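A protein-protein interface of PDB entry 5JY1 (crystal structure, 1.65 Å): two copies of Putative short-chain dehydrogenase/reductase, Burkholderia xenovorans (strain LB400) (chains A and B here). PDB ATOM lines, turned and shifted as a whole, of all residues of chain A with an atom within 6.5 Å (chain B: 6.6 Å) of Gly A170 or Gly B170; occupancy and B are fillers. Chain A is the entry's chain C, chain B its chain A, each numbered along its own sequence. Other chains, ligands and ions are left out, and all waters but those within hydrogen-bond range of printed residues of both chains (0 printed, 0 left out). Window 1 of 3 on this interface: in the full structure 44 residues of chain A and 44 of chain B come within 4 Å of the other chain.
Among the printed residues, pairs that only touch across the chains: Ala A169 with Ala B169, Leu A174 with Thr B166, Gly A170 with Thr B166, Thr A166 with Gly B170, Thr A166 with Leu B174, Thr A166 with Leu B124, Gly A173 with Ala B169, Ala A169 with Gly B173, Leu A124 with Thr B166, Gly A170 with Gly B170, Asn A165 with Gly B173 and Gly A173 with Asn B165.
Leu A124 touches Thr B166, and with the chains exchanged Thr A166 touches Leu B124. Thr A166 touches Gly B170, and with the chains exchanged Gly A170 touches Thr B166. Ala A169 touches its own counterpart, Ala B169. Gly A170 touches its own counterpart, Gly B170. Positions printed for both chains: 124, 154, 165, 166, 167, 168, 169, 170, 171, 172, 173, 174 and 175.
Printed residues of chain B within 4 Å of Gly A170: Thr B166 (3.4 Å) and Gly B170 (3.8 Å). Of the printed residues of chain B, Gly A173 touches Asn B165 (3.9 Å) and Ala B169 (3.6 Å). Of the printed residues of chain B, Leu A174 touches Thr B166. Of chain A, only Thr A166 (3.4 Å) and Gly A170 (3.8 Å) come within 4 Å of Gly B170. The nearest printed residue of chain B that does not touch Gly A173 is Thr B166 (4.2 Å).
Among the printed residues, 12 pairs touch across the chains.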
ATOM      1  N   LEU A 124     -23.686 -17.640  31.822  1.00  0.00           N
ATOM      2  CA  LEU A 124     -23.664 -16.431  31.013  1.00  0.00           C
ATOM      3  C   LEU A 124     -24.961 -15.636  31.143  1.00  0.00           C
ATOM      4  O   LEU A 124     -24.929 -14.441  31.459  1.00  0.00           O
ATOM      5  CB  LEU A 124     -23.372 -16.792  29.556  1.00  0.00           C
ATOM      6  CG  LEU A 124     -23.227 -15.588  28.642  1.00  0.00           C
ATOM      7  CD1 LEU A 124     -22.094 -14.682  29.143  1.00  0.00           C
ATOM      8  CD2 LEU A 124     -22.950 -16.054  27.226  1.00  0.00           C
ATOM      9  N   THR A 154     -10.829 -21.667  30.669  1.00  0.00           N
ATOM     10  CA  THR A 154     -11.117 -20.971  29.414  1.00  0.00           C
ATOM     11  C   THR A 154      -9.852 -20.668  28.647  1.00  0.00           C
ATOM     12  O   THR A 154      -9.917 -20.428  27.436  1.00  0.00           O
ATOM     13  CB  THR A 154     -11.837 -19.638  29.634  1.00  0.00           C
ATOM     14  OG1 THR A 154     -10.952 -18.726  30.299  1.00  0.00           O
ATOM     15  CG2 THR A 154     -13.067 -19.821  30.458  1.00  0.00           C
ATOM     16  N   ASN A 165     -16.035 -23.959  29.323  1.00  0.00           N
ATOM     17  CA  ASN A 165     -14.997 -23.078  28.783  1.00  0.00           C
ATOM     18  C   ASN A 165     -15.588 -22.045  27.833  1.00  0.00           C
ATOM     19  O   ASN A 165     -15.122 -20.896  27.770  1.00  0.00           O
ATOM     20  CB  ASN A 165     -13.937 -23.895  28.037  1.00  0.00           C
ATOM     21  CG  ASN A 165     -13.286 -24.960  28.895  1.00  0.00           C
ATOM     22  OD1 ASN A 165     -13.340 -24.910  30.131  1.00  0.00           O
ATOM     23  ND2 ASN A 165     -12.643 -25.932  28.244  1.00  0.00           N
ATOM     24  N   THR A 166     -16.596 -22.450  27.064  1.00  0.00           N
ATOM     25  CA  THR A 166     -17.247 -21.555  26.115  1.00  0.00           C
ATOM     26  C   THR A 166     -18.041 -20.478  26.839  1.00  0.00           C
ATOM     27  O   THR A 166     -17.884 -19.284  26.560  1.00  0.00           O
ATOM     28  CB  THR A 166     -18.151 -22.376  25.185  1.00  0.00           C
ATOM     29  OG1 THR A 166     -17.345 -23.316  24.450  1.00  0.00           O
ATOM     30  CG2 THR A 166     -18.893 -21.473  24.199  1.00  0.00           C
ATOM     31  N   ALA A 167     -18.897 -20.884  27.789  1.00  0.00           N
ATOM     32  CA  ALA A 167     -19.704 -19.904  28.515  1.00  0.00           C
ATOM     33  C   ALA A 167     -18.836 -18.949  29.328  1.00  0.00           C
ATOM     34  O   ALA A 167     -19.095 -17.739  29.366  1.00  0.00           O
ATOM     35  CB  ALA A 167     -20.707 -20.606  29.430  1.00  0.00           C
ATOM     36  N   LYS A 168     -17.814 -19.471  30.003  1.00  0.00           N
ATOM     37  CA  LYS A 168     -17.001 -18.601  30.841  1.00  0.00           C
ATOM     38  C   LYS A 168     -16.138 -17.669  29.999  1.00  0.00           C
ATOM     39  O   LYS A 168     -15.840 -16.547  30.429  1.00  0.00           O
ATOM     40  CB  LYS A 168     -16.153 -19.440  31.803  1.00  0.00           C
ATOM     41  CG  LYS A 168     -16.950 -20.211  32.884  1.00  0.00           C
ATOM     42  CD  LYS A 168     -17.684 -19.251  33.793  1.00  0.00           C
ATOM     43  CE  LYS A 168     -18.040 -19.838  35.158  1.00  0.00           C
ATOM     44  NZ  LYS A 168     -18.599 -18.739  36.017  1.00  0.00           N
ATOM     45  N   ALA A 169     -15.741 -18.091  28.795  1.00  0.00           N
ATOM     46  CA  ALA A 169     -15.084 -17.144  27.897  1.00  0.00           C
ATOM     47  C   ALA A 169     -16.052 -16.034  27.508  1.00  0.00           C
ATOM     48  O   ALA A 169     -15.671 -14.862  27.429  1.00  0.00           O
ATOM     49  CB  ALA A 169     -14.543 -17.864  26.655  1.00  0.00           C
ATOM     50  N   GLY A 170     -17.320 -16.380  27.272  1.00  0.00           N
ATOM     51  CA  GLY A 170     -18.303 -15.347  26.990  1.00  0.00           C
ATOM     52  C   GLY A 170     -18.416 -14.334  28.115  1.00  0.00           C
ATOM     53  O   GLY A 170     -18.598 -13.142  27.867  1.00  0.00           O
ATOM     54  N   ILE A 171     -18.289 -14.799  29.365  1.00  0.00           N
ATOM     55  CA  ILE A 171     -18.349 -13.890  30.507  1.00  0.00           C
ATOM     56  C   ILE A 171     -17.236 -12.848  30.433  1.00  0.00           C
ATOM     57  O   ILE A 171     -17.442 -11.685  30.804  1.00  0.00           O
ATOM     58  CB  ILE A 171     -18.306 -14.689  31.824  1.00  0.00           C
ATOM     59  CG1 ILE A 171     -19.668 -15.344  32.074  1.00  0.00           C
ATOM     60  CG2 ILE A 171     -17.878 -13.797  33.018  1.00  0.00           C
ATOM     61  CD1 ILE A 171     -19.678 -16.344  33.198  1.00  0.00           C
ATOM     62  N   VAL A 172     -16.051 -13.232  29.953  1.00  0.00           N
ATOM     63  CA  VAL A 172     -14.963 -12.254  29.819  1.00  0.00           C
ATOM     64  C   VAL A 172     -15.329 -11.178  28.797  1.00  0.00           C
ATOM     65  O   VAL A 172     -15.081  -9.982  29.011  1.00  0.00           O
ATOM     66  CB  VAL A 172     -13.637 -12.961  29.462  1.00  0.00           C
ATOM     67  CG1 VAL A 172     -12.527 -11.932  29.174  1.00  0.00           C
ATOM     68  CG2 VAL A 172     -13.197 -13.860  30.615  1.00  0.00           C
ATOM     69  N   GLY A 173     -15.920 -11.579  27.669  1.00  0.00           N
ATOM     70  CA  GLY A 173     -16.347 -10.587  26.689  1.00  0.00           C
ATOM     71  C   GLY A 173     -17.389  -9.634  27.246  1.00  0.00           C
ATOM     72  O   GLY A 173     -17.347  -8.426  26.990  1.00  0.00           O
ATOM     73  N   LEU A 174     -18.331 -10.164  28.036  1.00  0.00           N
ATOM     74  CA  LEU A 174     -19.355  -9.324  28.641  1.00  0.00           C
ATOM     75  C   LEU A 174     -18.756  -8.392  29.686  1.00  0.00           C
ATOM     76  O   LEU A 174     -19.150  -7.225  29.780  1.00  0.00           O
ATOM     77  CB  LEU A 174     -20.437 -10.210  29.254  1.00  0.00           C
ATOM     78  CG  LEU A 174     -21.555  -9.546  30.044  1.00  0.00           C
ATOM     79  CD1 LEU A 174     -22.284  -8.542  29.175  1.00  0.00           C
ATOM     80  CD2 LEU A 174     -22.523 -10.629  30.542  1.00  0.00           C
ATOM     81  N   THR A 175     -17.820  -8.906  30.493  1.00  0.00           N
ATOM     82  CA  THR A 175     -17.120  -8.084  31.480  1.00  0.00           C
ATOM     83  C   THR A 175     -16.451  -6.882  30.826  1.00  0.00           C
ATOM     84  O   THR A 175     -16.572  -5.746  31.301  1.00  0.00           O
ATOM     85  CB  THR A 175     -16.077  -8.950  32.195  1.00  0.00           C
ATOM     86  OG1 THR A 175     -16.737 -10.038  32.849  1.00  0.00           O
ATOM     87  CG2 THR A 175     -15.285  -8.140  33.238  1.00  0.00           C
ATOM     88  N   LEU B 124     -22.286 -18.306  17.993  1.00  0.00           N
ATOM     89  CA  LEU B 124     -21.738 -19.360  18.843  1.00  0.00           C
ATOM     90  C   LEU B 124     -22.338 -20.720  18.512  1.00  0.00           C
ATOM     91  O   LEU B 124     -21.602 -21.680  18.263  1.00  0.00           O
ATOM     92  CB  LEU B 124     -21.958 -19.011  20.317  1.00  0.00           C
ATOM     93  CG  LEU B 124     -21.299 -19.942  21.329  1.00  0.00           C
ATOM     94  CD1 LEU B 124     -19.805 -20.059  21.045  1.00  0.00           C
ATOM     95  CD2 LEU B 124     -21.545 -19.428  22.753  1.00  0.00           C
ATOM     96  N   THR B 154     -14.024  -8.011  20.998  1.00  0.00           N
ATOM     97  CA  THR B 154     -14.072  -8.802  22.229  1.00  0.00           C
ATOM     98  C   THR B 154     -12.971  -8.420  23.192  1.00  0.00           C
ATOM     99  O   THR B 154     -13.067  -8.742  24.382  1.00  0.00           O
ATOM    100  CB  THR B 154     -13.930 -10.304  21.958  1.00  0.00           C
ATOM    101  OG1 THR B 154     -12.589 -10.585  21.517  1.00  0.00           O
ATOM    102  CG2 THR B 154     -14.901 -10.757  20.905  1.00  0.00           C
ATOM    103  N   ASN B 165     -19.781  -8.966  21.339  1.00  0.00           N
ATOM    104  CA  ASN B 165     -18.538  -9.171  22.083  1.00  0.00           C
ATOM    105  C   ASN B 165     -18.617 -10.407  22.965  1.00  0.00           C
ATOM    106  O   ASN B 165     -17.639 -11.151  23.099  1.00  0.00           O
ATOM    107  CB  ASN B 165     -18.219  -7.947  22.953  1.00  0.00           C
ATOM    108  CG  ASN B 165     -18.100  -6.662  22.161  1.00  0.00           C
ATOM    109  OD1 ASN B 165     -17.867  -6.670  20.943  1.00  0.00           O
ATOM    110  ND2 ASN B 165     -18.256  -5.534  22.853  1.00  0.00           N
ATOM    111  N   THR B 166     -19.778 -10.630  23.585  1.00  0.00           N
ATOM    112  CA  THR B 166     -19.982 -11.798  24.434  1.00  0.00           C
ATOM    113  C   THR B 166     -19.937 -13.086  23.620  1.00  0.00           C
ATOM    114  O   THR B 166     -19.227 -14.034  23.975  1.00  0.00           O
ATOM    115  CB  THR B 166     -21.318 -11.653  25.156  1.00  0.00           C
ATOM    116  OG1 THR B 166     -21.255 -10.499  26.007  1.00  0.00           O
ATOM    117  CG2 THR B 166     -21.632 -12.891  25.988  1.00  0.00           C
ATOM    118  N   ALA B 167     -20.683 -13.132  22.515  1.00  0.00           N
ATOM    119  CA  ALA B 167     -20.742 -14.356  21.715  1.00  0.00           C
ATOM    120  C   ALA B 167     -19.391 -14.675  21.086  1.00  0.00           C
ATOM    121  O   ALA B 167     -18.953 -15.833  21.098  1.00  0.00           O
ATOM    122  CB  ALA B 167     -21.817 -14.229  20.637  1.00  0.00           C
ATOM    123  N   LYS B 168     -18.706 -13.660  20.551  1.00  0.00           N
ATOM    124  CA  LYS B 168     -17.412 -13.905  19.915  1.00  0.00           C
ATOM    125  C   LYS B 168     -16.336 -14.261  20.939  1.00  0.00           C
ATOM    126  O   LYS B 168     -15.406 -15.016  20.624  1.00  0.00           O
ATOM    127  CB  LYS B 168     -16.996 -12.689  19.080  1.00  0.00           C
ATOM    128  CG  LYS B 168     -17.855 -12.427  17.829  1.00  0.00           C
ATOM    129  CD  LYS B 168     -17.752 -13.571  16.827  1.00  0.00           C
ATOM    130  CE  LYS B 168     -18.175 -13.115  15.430  1.00  0.00           C
ATOM    131  NZ  LYS B 168     -17.919 -14.175  14.402  1.00  0.00           N
ATOM    132  N   ALA B 169     -16.449 -13.760  22.173  1.00  0.00           N
ATOM    133  CA  ALA B 169     -15.565 -14.244  23.227  1.00  0.00           C
ATOM    134  C   ALA B 169     -15.798 -15.729  23.493  1.00  0.00           C
ATOM    135  O   ALA B 169     -14.840 -16.496  23.663  1.00  0.00           O
ATOM    136  CB  ALA B 169     -15.768 -13.424  24.507  1.00  0.00           C
ATOM    137  N   GLY B 170     -17.065 -16.153  23.527  1.00  0.00           N
ATOM    138  CA  GLY B 170     -17.358 -17.576  23.646  1.00  0.00           C
ATOM    139  C   GLY B 170     -16.695 -18.406  22.559  1.00  0.00           C
ATOM    140  O   GLY B 170     -16.221 -19.519  22.815  1.00  0.00           O
ATOM    141  N   ILE B 171     -16.637 -17.867  21.337  1.00  0.00           N
ATOM    142  CA  ILE B 171     -15.987 -18.567  20.226  1.00  0.00           C
ATOM    143  C   ILE B 171     -14.535 -18.883  20.565  1.00  0.00           C
ATOM    144  O   ILE B 171     -14.017 -19.953  20.223  1.00  0.00           O
ATOM    145  CB  ILE B 171     -16.087 -17.728  18.936  1.00  0.00           C
ATOM    146  CG1 ILE B 171     -17.537 -17.605  18.479  1.00  0.00           C
ATOM    147  CG2 ILE B 171     -15.225 -18.335  17.830  1.00  0.00           C
ATOM    148  CD1 ILE B 171     -18.102 -18.890  17.937  1.00  0.00           C
ATOM    149  N   VAL B 172     -13.845 -17.950  21.228  1.00  0.00           N
ATOM    150  CA  VAL B 172     -12.452 -18.195  21.597  1.00  0.00           C
ATOM    151  C   VAL B 172     -12.346 -19.347  22.591  1.00  0.00           C
ATOM    152  O   VAL B 172     -11.469 -20.213  22.468  1.00  0.00           O
ATOM    153  CB  VAL B 172     -11.804 -16.909  22.146  1.00  0.00           C
ATOM    154  CG1 VAL B 172     -10.386 -17.198  22.626  1.00  0.00           C
ATOM    155  CG2 VAL B 172     -11.798 -15.820  21.080  1.00  0.00           C
ATOM    156  N   GLY B 173     -13.235 -19.384  23.587  1.00  0.00           N
ATOM    157  CA  GLY B 173     -13.212 -20.495  24.525  1.00  0.00           C
ATOM    158  C   GLY B 173     -13.483 -21.827  23.847  1.00  0.00           C
ATOM    159  O   GLY B 173     -12.845 -22.835  24.161  1.00  0.00           O
ATOM    160  N   LEU B 174     -14.425 -21.841  22.896  1.00  0.00           N
ATOM    161  CA  LEU B 174     -14.737 -23.066  22.164  1.00  0.00           C
ATOM    162  C   LEU B 174     -13.564 -23.491  21.285  1.00  0.00           C
ATOM    163  O   LEU B 174     -13.249 -24.686  21.196  1.00  0.00           O
ATOM    164  CB  LEU B 174     -15.999 -22.846  21.331  1.00  0.00           C
ATOM    165  CG  LEU B 174     -16.465 -24.009  20.447  1.00  0.00           C
ATOM    166  CD1 LEU B 174     -16.649 -25.279  21.279  1.00  0.00           C
ATOM    167  CD2 LEU B 174     -17.760 -23.622  19.729  1.00  0.00           C
ATOM    168  N   THR B 175     -12.900 -22.517  20.653  1.00  0.00           N
ATOM    169  CA  THR B 175     -11.726 -22.788  19.828  1.00  0.00           C
ATOM    170  C   THR B 175     -10.630 -23.471  20.639  1.00  0.00           C
ATOM    171  O   THR B 175     -10.074 -24.497  20.233  1.00  0.00           O
ATOM    172  CB  THR B 175     -11.205 -21.472  19.240  1.00  0.00           C
ATOM    173  OG1 THR B 175     -12.217 -20.882  18.411  1.00  0.00           O
ATOM    174  CG2 THR B 175      -9.918 -21.700  18.421  1.00  0.00           C
